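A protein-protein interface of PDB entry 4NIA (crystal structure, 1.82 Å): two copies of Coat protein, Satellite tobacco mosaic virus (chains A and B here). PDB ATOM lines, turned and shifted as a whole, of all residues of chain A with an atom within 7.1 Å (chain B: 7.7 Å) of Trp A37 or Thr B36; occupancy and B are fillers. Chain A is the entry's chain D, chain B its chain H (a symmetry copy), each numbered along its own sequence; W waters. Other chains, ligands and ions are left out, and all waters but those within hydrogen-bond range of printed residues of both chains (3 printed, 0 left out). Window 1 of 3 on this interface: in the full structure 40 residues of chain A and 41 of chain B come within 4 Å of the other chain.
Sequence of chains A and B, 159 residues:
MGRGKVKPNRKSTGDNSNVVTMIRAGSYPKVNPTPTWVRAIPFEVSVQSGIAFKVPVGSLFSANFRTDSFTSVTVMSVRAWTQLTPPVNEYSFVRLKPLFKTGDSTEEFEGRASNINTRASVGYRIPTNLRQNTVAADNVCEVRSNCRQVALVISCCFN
O of Pro A35 sits at hydrogen-bond distance from NE of Arg B66 (2.9 Å).
NH2 of Arg A39 sits at hydrogen-bond distance from O of Pro B33, 2.8 Å away.
The guanidinium group (NH2) of Arg A66 lies within hydrogen-bond range of the backbone carbonyl oxygen (O) of Thr B34 (3.1 Å).
The guanidinium group (NE) of Arg A66 is in hydrogen-bond range of the backbone carbonyl oxygen (O) of Pro B35 (2.9 Å).
The side-chain hydroxyl (OG) of Ser B69 lies within hydrogen-bond range of the guanidinium group (NH1) of Arg A66, at 2.9 Å.
The backbone carbonyl oxygen of Pro B33 lies close to the backbone carbonyl oxygen of Phe A65, at 3.5 Å.
The backbone NH of Phe A158 sits at hydrogen-bond distance from the backbone carbonyl oxygen of Trp A37, 2.8 Å away.
NH1 of Arg A39 sits at hydrogen-bond distance from O of Phe A65.
N of Arg A39 lies within hydrogen-bond range of O of Cys A156 (2.8 Å).
OD1 of Asn B32 is in hydrogen-bond range of N of Thr B34.
The backbone carbonyl oxygen of Trp B37 lies within hydrogen-bond range of the backbone NH of Phe B158 (2.9 Å).
Among the printed residues, merely in contact across the chains: Phe A70 with Arg B66, Arg A39 with Pro B35, Arg A66 with Phe B70, Pro A35 with Arg B39, Trp A37 with Trp B37, Trp A37 with Thr B36 and Thr A36 with Trp B37.
Of chain B, only Thr B36 and Trp B37 come within 4 Å of Trp A37.
Thr B36 touches just one residue of chain A: Trp A37 (3.8 Å).
Of the printed residues of chain B, Phe A65 touches Pro B33 (3.2 Å).
Of the printed residues of chain A, Trp B37 touches Thr A36 and Trp A37.
Of the printed residues of chain B, Arg A66 touches Thr B34, Pro B35, Ser B69 and Phe B70.
The nearest residue of chain B that does not touch Trp A37 is Pro B35 (4.1 Å).
The nearest residue of chain A that does not touch Thr B36 is Arg A66 (5.1 Å).
The nearest printed residue of chain A that does not touch Arg B39 is Thr A36 (6.7 Å).
Of the 15 printed residues of chain B, 9 touch a printed residue of chain A.
Of the 14 printed residues of chain A, 7 touch a printed residue of chain B.
Printed residues of chain A that touch a printed residue of chain B: Pro A35, Thr A36, Trp A37, Arg A39, Phe A65, Arg A66 and Phe A70.
Hydrophobic or aromatic side chains of chain A within 4 Å of the printed part of chain B: Pro A35, Trp A37, Phe A65 and Phe A70.
Pro A35 touches Arg B66, and with the chains exchanged Arg A66 touches Pro B35.
Thr A36 touches Trp B37, and with the chains exchanged Trp A37 touches Thr B36.
Trp A37 touches its own counterpart, Trp B37.
Arg A66 touches Phe B70, and with the chains exchanged Phe A70 touches Arg B66.
Positions printed for both chains: 35, 36, 37, 38, 39, 66, 67, 70, 157, 158 and 159.
Of the 13 pairs that touch across the chains among the printed residues, 9 have their exchanged pair printed and touching as well.
Water W2 lies within hydrogen-bond range of O of Asn B32 (2.7 Å) and NH2 of Arg A39 (2.8 Å).
Water W1 bridges O of Thr A36 (2.8 Å) and NE1 of Trp B37 (2.9 Å).
Water W3 bridges the backbone carbonyl oxygen of Thr B36 (2.8 Å) and the indole nitrogen of Trp A37 (3.0 Å).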
ATOM      1  N   PRO A  35     -10.039  16.122 -16.186  1.00  0.00           N
ATOM      2  CA  PRO A  35     -11.489  16.262 -16.089  1.00  0.00           C
ATOM      3  C   PRO A  35     -12.133  15.295 -15.117  1.00  0.00           C
ATOM      4  O   PRO A  35     -11.481  14.374 -14.597  1.00  0.00           O
ATOM      5  CB  PRO A  35     -11.986  15.941 -17.500  1.00  0.00           C
ATOM      6  CG  PRO A  35     -10.893  15.136 -18.127  1.00  0.00           C
ATOM      7  CD  PRO A  35      -9.626  15.377 -17.396  1.00  0.00           C
ATOM      8  N   THR A  36     -13.423  15.518 -14.909  1.00  0.00           N
ATOM      9  CA  THR A  36     -14.272  14.637 -14.119  1.00  0.00           C
ATOM     10  C   THR A  36     -14.607  13.378 -14.924  1.00  0.00           C
ATOM     11  O   THR A  36     -14.358  13.304 -16.132  1.00  0.00           O
ATOM     12  CB  THR A  36     -15.616  15.336 -13.807  1.00  0.00           C
ATOM     13  OG1 THR A  36     -16.226  15.751 -15.039  1.00  0.00           O
ATOM     14  CG2 THR A  36     -15.373  16.574 -12.901  1.00  0.00           C
ATOM     15  N   TRP A  37     -15.201  12.395 -14.262  1.00  0.00           N
ATOM     16  CA  TRP A  37     -15.467  11.099 -14.904  1.00  0.00           C
ATOM     17  C   TRP A  37     -16.587  10.401 -14.171  1.00  0.00           C
ATOM     18  O   TRP A  37     -16.476  10.125 -12.968  1.00  0.00           O
ATOM     19  CB  TRP A  37     -14.229  10.214 -14.869  1.00  0.00           C
ATOM     20  CG  TRP A  37     -14.144   9.176 -15.999  1.00  0.00           C
ATOM     21  CD1 TRP A  37     -15.038   8.945 -16.991  1.00  0.00           C
ATOM     22  CD2 TRP A  37     -13.056   8.280 -16.228  1.00  0.00           C
ATOM     23  NE1 TRP A  37     -14.592   7.952 -17.820  1.00  0.00           N
ATOM     24  CE2 TRP A  37     -13.374   7.524 -17.376  1.00  0.00           C
ATOM     25  CE3 TRP A  37     -11.862   8.030 -15.565  1.00  0.00           C
ATOM     26  CZ2 TRP A  37     -12.506   6.574 -17.905  1.00  0.00           C
ATOM     27  CZ3 TRP A  37     -10.995   7.091 -16.098  1.00  0.00           C
ATOM     28  CH2 TRP A  37     -11.319   6.396 -17.255  1.00  0.00           C
ATOM     29  N   VAL A  38     -17.650  10.073 -14.905  1.00  0.00           N
ATOM     30  CA  VAL A  38     -18.774   9.320 -14.363  1.00  0.00           C
ATOM     31  C   VAL A  38     -18.534   7.830 -14.609  1.00  0.00           C
ATOM     32  O   VAL A  38     -18.248   7.425 -15.733  1.00  0.00           O
ATOM     33  CB  VAL A  38     -20.105   9.746 -15.017  1.00  0.00           C
ATOM     34  CG1 VAL A  38     -21.263   8.902 -14.482  1.00  0.00           C
ATOM     35  CG2 VAL A  38     -20.365  11.216 -14.715  1.00  0.00           C
ATOM     36  N   ARG A  39     -18.629   7.029 -13.554  1.00  0.00           N
ATOM     37  CA  ARG A  39     -18.181   5.640 -13.576  1.00  0.00           C
ATOM     38  C   ARG A  39     -19.111   4.680 -12.835  1.00  0.00           C
ATOM     39  O   ARG A  39     -19.804   5.072 -11.914  1.00  0.00           O
ATOM     40  CB  ARG A  39     -16.782   5.504 -12.979  1.00  0.00           C
ATOM     41  CG  ARG A  39     -15.687   6.302 -13.706  1.00  0.00           C
ATOM     42  CD  ARG A  39     -15.279   5.655 -15.013  1.00  0.00           C
ATOM     43  NE  ARG A  39     -14.824   4.288 -14.783  1.00  0.00           N
ATOM     44  CZ  ARG A  39     -13.574   3.974 -14.449  1.00  0.00           C
ATOM     45  NH1 ARG A  39     -12.661   4.918 -14.336  1.00  0.00           N
ATOM     46  NH2 ARG A  39     -13.252   2.722 -14.216  1.00  0.00           N
ATOM     47  N   PHE A  65      -8.646   0.825 -11.648  1.00  0.00           N
ATOM     48  CA  PHE A  65      -9.840   1.432 -12.228  1.00  0.00           C
ATOM     49  C   PHE A  65      -9.549   2.687 -13.046  1.00  0.00           C
ATOM     50  O   PHE A  65     -10.462   3.330 -13.539  1.00  0.00           O
ATOM     51  CB  PHE A  65     -10.819   1.812 -11.106  1.00  0.00           C
ATOM     52  CG  PHE A  65     -11.162   0.683 -10.177  1.00  0.00           C
ATOM     53  CD1 PHE A  65     -11.548  -0.562 -10.654  1.00  0.00           C
ATOM     54  CD2 PHE A  65     -11.095   0.869  -8.806  1.00  0.00           C
ATOM     55  CE1 PHE A  65     -11.879  -1.589  -9.775  1.00  0.00           C
ATOM     56  CE2 PHE A  65     -11.395  -0.160  -7.932  1.00  0.00           C
ATOM     57  CZ  PHE A  65     -11.782  -1.388  -8.409  1.00  0.00           C
ATOM     58  N   ARG A  66      -8.275   3.004 -13.205  1.00  0.00           N
ATOM     59  CA  ARG A  66      -7.831   4.251 -13.810  1.00  0.00           C
ATOM     60  C   ARG A  66      -8.176   5.491 -12.981  1.00  0.00           C
ATOM     61  O   ARG A  66      -8.288   6.582 -13.529  1.00  0.00           O
ATOM     62  CB  ARG A  66      -8.404   4.379 -15.249  1.00  0.00           C
ATOM     63  CG  ARG A  66      -8.312   3.152 -16.117  1.00  0.00           C
ATOM     64  CD  ARG A  66      -8.694   3.563 -17.543  1.00  0.00           C
ATOM     65  NE  ARG A  66      -8.923   2.537 -18.540  1.00  0.00           N
ATOM     66  CZ  ARG A  66      -7.986   1.838 -19.175  1.00  0.00           C
ATOM     67  NH1 ARG A  66      -6.703   1.962 -18.861  1.00  0.00           N
ATOM     68  NH2 ARG A  66      -8.336   1.044 -20.186  1.00  0.00           N
ATOM     69  N   THR A  67      -8.341   5.336 -11.660  1.00  0.00           N
ATOM     70  CA  THR A  67      -8.831   6.434 -10.838  1.00  0.00           C
ATOM     71  C   THR A  67      -7.873   6.892  -9.723  1.00  0.00           C
ATOM     72  O   THR A  67      -8.252   7.653  -8.859  1.00  0.00           O
ATOM     73  CB  THR A  67     -10.145   6.026 -10.162  1.00  0.00           C
ATOM     74  OG1 THR A  67      -9.924   4.806  -9.451  1.00  0.00           O
ATOM     75  CG2 THR A  67     -11.229   5.823 -11.214  1.00  0.00           C
ATOM     76  N   PHE A  70      -7.479  10.797  -8.774  1.00  0.00           N
ATOM     77  CA  PHE A  70      -8.538  11.538  -8.098  1.00  0.00           C
ATOM     78  C   PHE A  70      -8.366  11.436  -6.574  1.00  0.00           C
ATOM     79  O   PHE A  70      -7.849  10.449  -6.058  1.00  0.00           O
ATOM     80  CB  PHE A  70      -9.897  10.987  -8.453  1.00  0.00           C
ATOM     81  CG  PHE A  70     -10.281  11.186  -9.877  1.00  0.00           C
ATOM     82  CD1 PHE A  70     -10.122  10.175 -10.797  1.00  0.00           C
ATOM     83  CD2 PHE A  70     -10.882  12.376 -10.279  1.00  0.00           C
ATOM     84  CE1 PHE A  70     -10.514  10.335 -12.117  1.00  0.00           C
ATOM     85  CE2 PHE A  70     -11.267  12.555 -11.601  1.00  0.00           C
ATOM     86  CZ  PHE A  70     -11.070  11.537 -12.522  1.00  0.00           C
ATOM     87  N   VAL A  73     -14.679  11.826  -4.630  1.00  0.00           N
ATOM     88  CA  VAL A  73     -15.710  11.200  -5.422  1.00  0.00           C
ATOM     89  C   VAL A  73     -17.089  11.520  -4.860  1.00  0.00           C
ATOM     90  O   VAL A  73     -17.282  11.681  -3.635  1.00  0.00           O
ATOM     91  CB  VAL A  73     -15.435   9.672  -5.561  1.00  0.00           C
ATOM     92  CG1 VAL A  73     -15.543   8.959  -4.224  1.00  0.00           C
ATOM     93  CG2 VAL A  73     -16.361   9.031  -6.569  1.00  0.00           C
ATOM     94  N   CYS A 156     -20.796   6.523  -9.601  1.00  0.00           N
ATOM     95  CA  CYS A 156     -20.193   7.671  -8.971  1.00  0.00           C
ATOM     96  C   CYS A 156     -19.550   8.625  -9.966  1.00  0.00           C
ATOM     97  O   CYS A 156     -19.337   8.287 -11.142  1.00  0.00           O
ATOM     98  CB  CYS A 156     -19.192   7.224  -7.915  1.00  0.00           C
ATOM     99  SG  CYS A 156     -17.848   6.194  -8.512  1.00  0.00           S
ATOM    100  N   CYS A 157     -19.279   9.828  -9.476  1.00  0.00           N
ATOM    101  CA  CYS A 157     -18.643  10.887 -10.256  1.00  0.00           C
ATOM    102  C   CYS A 157     -17.317  11.275  -9.604  1.00  0.00           C
ATOM    103  O   CYS A 157     -17.310  11.924  -8.527  1.00  0.00           O
ATOM    104  CB  CYS A 157     -19.524  12.150 -10.286  1.00  0.00           C
ATOM    105  SG  CYS A 157     -21.246  11.860 -10.761  1.00  0.00           S
ATOM    106  N   PHE A 158     -16.216  10.921 -10.271  1.00  0.00           N
ATOM    107  CA  PHE A 158     -14.893  11.279  -9.817  1.00  0.00           C
ATOM    108  C   PHE A 158     -14.613  12.730 -10.182  1.00  0.00           C
ATOM    109  O   PHE A 158     -14.923  13.163 -11.282  1.00  0.00           O
ATOM    110  CB  PHE A 158     -13.850  10.368 -10.435  1.00  0.00           C
ATOM    111  CG  PHE A 158     -13.872   8.981  -9.880  1.00  0.00           C
ATOM    112  CD1 PHE A 158     -13.143   8.667  -8.736  1.00  0.00           C
ATOM    113  CD2 PHE A 158     -14.642   8.004 -10.463  1.00  0.00           C
ATOM    114  CE1 PHE A 158     -13.155   7.380  -8.230  1.00  0.00           C
ATOM    115  CE2 PHE A 158     -14.660   6.730  -9.945  1.00  0.00           C
ATOM    116  CZ  PHE A 158     -13.913   6.416  -8.827  1.00  0.00           C
ATOM    117  N   ASN A 159     -14.130  13.496  -9.217  1.00  0.00           N
ATOM    118  CA  ASN A 159     -13.818  14.901  -9.478  1.00  0.00           C
ATOM    119  C   ASN A 159     -12.602  15.334  -8.669  1.00  0.00           C
ATOM    120  O   ASN A 159     -11.888  16.289  -9.014  1.00  0.00           O
ATOM    121  CB  ASN A 159     -15.030  15.792  -9.215  1.00  0.00           C
ATOM    122  CG  ASN A 159     -15.417  15.844  -7.751  1.00  0.00           C
ATOM    123  OD1 ASN A 159     -15.105  16.800  -7.042  1.00  0.00           O
ATOM    124  ND2 ASN A 159     -16.142  14.828  -7.300  1.00  0.00           N
ATOM    125  OXT ASN A 159     -12.311  14.688  -7.666  1.00  0.00           O
ATOM    126  N   ASN B  32     -16.816  -3.513 -16.390  1.00  0.00           N
ATOM    127  CA  ASN B  32     -15.483  -3.258 -16.948  1.00  0.00           C
ATOM    128  C   ASN B  32     -14.790  -2.225 -16.082  1.00  0.00           C
ATOM    129  O   ASN B  32     -15.180  -1.050 -16.073  1.00  0.00           O
ATOM    130  CB  ASN B  32     -15.579  -2.744 -18.389  1.00  0.00           C
ATOM    131  CG  ASN B  32     -14.216  -2.446 -18.996  1.00  0.00           C
ATOM    132  OD1 ASN B  32     -13.180  -2.861 -18.476  1.00  0.00           O
ATOM    133  ND2 ASN B  32     -14.220  -1.695 -20.076  1.00  0.00           N
ATOM    134  N   PRO B  33     -13.736  -2.642 -15.370  1.00  0.00           N
ATOM    135  CA  PRO B  33     -13.043  -1.774 -14.433  1.00  0.00           C
ATOM    136  C   PRO B  33     -12.168  -0.729 -15.122  1.00  0.00           C
ATOM    137  O   PRO B  33     -11.831   0.287 -14.516  1.00  0.00           O
ATOM    138  CB  PRO B  33     -12.146  -2.745 -13.639  1.00  0.00           C
ATOM    139  CG  PRO B  33     -11.992  -3.934 -14.472  1.00  0.00           C
ATOM    140  CD  PRO B  33     -13.245  -4.036 -15.316  1.00  0.00           C
ATOM    141  N   THR B  34     -11.868  -0.949 -16.400  1.00  0.00           N
ATOM    142  CA  THR B  34     -10.907  -0.139 -17.156  1.00  0.00           C
ATOM    143  C   THR B  34     -11.469   0.295 -18.523  1.00  0.00           C
ATOM    144  O   THR B  34     -11.129  -0.270 -19.562  1.00  0.00           O
ATOM    145  CB  THR B  34      -9.586  -0.914 -17.341  1.00  0.00           C
ATOM    146  OG1 THR B  34      -9.861  -2.268 -17.700  1.00  0.00           O
ATOM    147  CG2 THR B  34      -8.764  -0.924 -16.057  1.00  0.00           C
ATOM    148  N   PRO B  35     -12.368   1.285 -18.519  1.00  0.00           N
ATOM    149  CA  PRO B  35     -13.019   1.691 -19.746  1.00  0.00           C
ATOM    150  C   PRO B  35     -12.215   2.615 -20.647  1.00  0.00           C
ATOM    151  O   PRO B  35     -11.120   3.099 -20.295  1.00  0.00           O
ATOM    152  CB  PRO B  35     -14.289   2.411 -19.273  1.00  0.00           C
ATOM    153  CG  PRO B  35     -14.023   2.811 -17.870  1.00  0.00           C
ATOM    154  CD  PRO B  35     -12.944   1.929 -17.330  1.00  0.00           C
ATOM    155  N   THR B  36     -12.812   2.845 -21.811  1.00  0.00           N
ATOM    156  CA  THR B  36     -12.282   3.776 -22.780  1.00  0.00           C
ATOM    157  C   THR B  36     -12.606   5.196 -22.346  1.00  0.00           C
ATOM    158  O   THR B  36     -13.402   5.421 -21.418  1.00  0.00           O
ATOM    159  CB  THR B  36     -12.925   3.540 -24.149  1.00  0.00           C
ATOM    160  OG1 THR B  36     -14.355   3.622 -24.013  1.00  0.00           O
ATOM    161  CG2 THR B  36     -12.516   2.159 -24.684  1.00  0.00           C
ATOM    162  N   TRP B  37     -11.990   6.172 -23.000  1.00  0.00           N
ATOM    163  CA  TRP B  37     -12.240   7.587 -22.599  1.00  0.00           C
ATOM    164  C   TRP B  37     -11.965   8.487 -23.784  1.00  0.00           C
ATOM    165  O   TRP B  37     -10.869   8.439 -24.363  1.00  0.00           O
ATOM    166  CB  TRP B  37     -11.287   7.977 -21.480  1.00  0.00           C
ATOM    167  CG  TRP B  37     -11.759   9.058 -20.575  1.00  0.00           C
ATOM    168  CD1 TRP B  37     -12.911   9.787 -20.668  1.00  0.00           C
ATOM    169  CD2 TRP B  37     -11.083   9.526 -19.406  1.00  0.00           C
ATOM    170  NE1 TRP B  37     -12.984  10.675 -19.640  1.00  0.00           N
ATOM    171  CE2 TRP B  37     -11.877  10.544 -18.850  1.00  0.00           C
ATOM    172  CE3 TRP B  37      -9.879   9.192 -18.795  1.00  0.00           C
ATOM    173  CZ2 TRP B  37     -11.538  11.193 -17.674  1.00  0.00           C
ATOM    174  CZ3 TRP B  37      -9.539   9.839 -17.615  1.00  0.00           C
ATOM    175  CH2 TRP B  37     -10.372  10.830 -17.075  1.00  0.00           C
ATOM    176  N   VAL B  38     -12.947   9.311 -24.138  1.00  0.00           N
ATOM    177  CA  VAL B  38     -12.786  10.287 -25.195  1.00  0.00           C
ATOM    178  C   VAL B  38     -12.338  11.609 -24.599  1.00  0.00           C
ATOM    179  O   VAL B  38     -12.941  12.092 -23.626  1.00  0.00           O
ATOM    180  CB  VAL B  38     -14.100  10.456 -25.968  1.00  0.00           C
ATOM    181  CG1 VAL B  38     -13.950  11.503 -27.080  1.00  0.00           C
ATOM    182  CG2 VAL B  38     -14.538   9.127 -26.571  1.00  0.00           C
ATOM    183  N   ARG B  39     -11.270  12.187 -25.156  1.00  0.00           N
ATOM    184  CA  ARG B  39     -10.579  13.275 -24.484  1.00  0.00           C
ATOM    185  C   ARG B  39     -10.101  14.338 -25.471  1.00  0.00           C
ATOM    186  O   ARG B  39      -9.878  14.051 -26.627  1.00  0.00           O
ATOM    187  CB  ARG B  39      -9.358  12.725 -23.716  1.00  0.00           C
ATOM    188  CG  ARG B  39      -9.692  11.807 -22.560  1.00  0.00           C
ATOM    189  CD  ARG B  39     -10.331  12.551 -21.387  1.00  0.00           C
ATOM    190  NE  ARG B  39      -9.426  13.561 -20.868  1.00  0.00           N
ATOM    191  CZ  ARG B  39      -8.422  13.322 -20.025  1.00  0.00           C
ATOM    192  NH1 ARG B  39      -8.218  12.106 -19.561  1.00  0.00           N
ATOM    193  NH2 ARG B  39      -7.565  14.283 -19.721  1.00  0.00           N
ATOM    194  N   ARG B  66      -4.429  12.154 -16.326  1.00  0.00           N
ATOM    195  CA  ARG B  66      -5.113  10.943 -15.864  1.00  0.00           C
ATOM    196  C   ARG B  66      -5.090   9.769 -16.876  1.00  0.00           C
ATOM    197  O   ARG B  66      -5.944   8.865 -16.851  1.00  0.00           O
ATOM    198  CB  ARG B  66      -6.571  11.249 -15.514  1.00  0.00           C
ATOM    199  CG  ARG B  66      -6.804  12.568 -14.786  1.00  0.00           C
ATOM    200  CD  ARG B  66      -8.223  12.556 -14.235  1.00  0.00           C
ATOM    201  NE  ARG B  66      -8.771  13.794 -13.682  1.00  0.00           N
ATOM    202  CZ  ARG B  66      -8.623  14.192 -12.416  1.00  0.00           C
ATOM    203  NH1 ARG B  66      -7.763  13.586 -11.622  1.00  0.00           N
ATOM    204  NH2 ARG B  66      -9.252  15.254 -11.988  1.00  0.00           N
ATOM    205  N   THR B  67      -4.110   9.752 -17.759  1.00  0.00           N
ATOM    206  CA  THR B  67      -4.092   8.741 -18.818  1.00  0.00           C
ATOM    207  C   THR B  67      -2.885   7.791 -18.783  1.00  0.00           C
ATOM    208  O   THR B  67      -2.664   7.070 -19.735  1.00  0.00           O
ATOM    209  CB  THR B  67      -4.055   9.415 -20.164  1.00  0.00           C
ATOM    210  OG1 THR B  67      -2.921  10.280 -20.201  1.00  0.00           O
ATOM    211  CG2 THR B  67      -5.337  10.218 -20.414  1.00  0.00           C
ATOM    212  N   SER B  69      -2.600   4.969 -17.326  1.00  0.00           N
ATOM    213  CA  SER B  69      -2.997   3.552 -17.326  1.00  0.00           C
ATOM    214  C   SER B  69      -3.298   3.008 -18.737  1.00  0.00           C
ATOM    215  O   SER B  69      -3.540   1.804 -18.911  1.00  0.00           O
ATOM    216  CB  SER B  69      -4.205   3.296 -16.437  1.00  0.00           C
ATOM    217  OG  SER B  69      -5.377   3.829 -17.014  1.00  0.00           O
ATOM    218  N   PHE B  70      -3.294   3.884 -19.727  1.00  0.00           N
ATOM    219  CA  PHE B  70      -3.504   3.479 -21.112  1.00  0.00           C
ATOM    220  C   PHE B  70      -2.169   3.246 -21.820  1.00  0.00           C
ATOM    221  O   PHE B  70      -1.173   3.915 -21.518  1.00  0.00           O
ATOM    222  CB  PHE B  70      -4.295   4.533 -21.878  1.00  0.00           C
ATOM    223  CG  PHE B  70      -5.699   4.721 -21.387  1.00  0.00           C
ATOM    224  CD1 PHE B  70      -6.021   5.803 -20.583  1.00  0.00           C
ATOM    225  CD2 PHE B  70      -6.722   3.903 -21.836  1.00  0.00           C
ATOM    226  CE1 PHE B  70      -7.339   6.022 -20.179  1.00  0.00           C
ATOM    227  CE2 PHE B  70      -8.045   4.138 -21.456  1.00  0.00           C
ATOM    228  CZ  PHE B  70      -8.328   5.171 -20.587  1.00  0.00           C
ATOM    229  N   CYS B 157      -9.343   9.036 -28.560  1.00  0.00           N
ATOM    230  CA  CYS B 157     -10.012   7.971 -27.824  1.00  0.00           C
ATOM    231  C   CYS B 157      -8.973   7.043 -27.210  1.00  0.00           C
ATOM    232  O   CYS B 157      -8.320   6.248 -27.898  1.00  0.00           O
ATOM    233  CB  CYS B 157     -10.907   7.166 -28.762  1.00  0.00           C
ATOM    234  SG  CYS B 157     -12.039   8.160 -29.730  1.00  0.00           S
ATOM    235  N   PHE B 158      -8.827   7.127 -25.896  1.00  0.00           N
ATOM    236  CA  PHE B 158      -7.947   6.239 -25.186  1.00  0.00           C
ATOM    237  C   PHE B 158      -8.622   4.909 -25.019  1.00  0.00           C
ATOM    238  O   PHE B 158      -9.826   4.838 -24.772  1.00  0.00           O
ATOM    239  CB  PHE B 158      -7.628   6.846 -23.807  1.00  0.00           C
ATOM    240  CG  PHE B 158      -6.690   7.994 -23.882  1.00  0.00           C
ATOM    241  CD1 PHE B 158      -5.300   7.793 -23.931  1.00  0.00           C
ATOM    242  CD2 PHE B 158      -7.182   9.276 -23.948  1.00  0.00           C
ATOM    243  CE1 PHE B 158      -4.442   8.853 -24.067  1.00  0.00           C
ATOM    244  CE2 PHE B 158      -6.318  10.354 -24.042  1.00  0.00           C
ATOM    245  CZ  PHE B 158      -4.953  10.140 -24.118  1.00  0.00           C
ATOM    246  N   ASN B 159      -7.859   3.848 -25.209  1.00  0.00           N
ATOM    247  CA  ASN B 159      -8.409   2.504 -25.103  1.00  0.00           C
ATOM    248  C   ASN B 159      -7.348   1.519 -24.683  1.00  0.00           C
ATOM    249  O   ASN B 159      -7.675   0.460 -24.135  1.00  0.00           O
ATOM    250  CB  ASN B 159      -9.123   2.058 -26.398  1.00  0.00           C
ATOM    251  CG  ASN B 159      -8.191   1.852 -27.570  1.00  0.00           C
ATOM    252  OD1 ASN B 159      -7.797   0.734 -27.896  1.00  0.00           O
ATOM    253  ND2 ASN B 159      -7.861   2.923 -28.229  1.00  0.00           N
ATOM    254  OXT ASN B 159      -6.160   1.790 -24.856  1.00  0.00           O
HETATM  255  O   HOH W   1     -15.097  12.341 -18.617  1.00  0.00           O
HETATM  256  O   HOH W   2     -15.392   0.942 -14.261  1.00  0.00           O
HETATM  257  O   HOH W   3     -15.464   7.032 -20.520  1.00  0.00           O
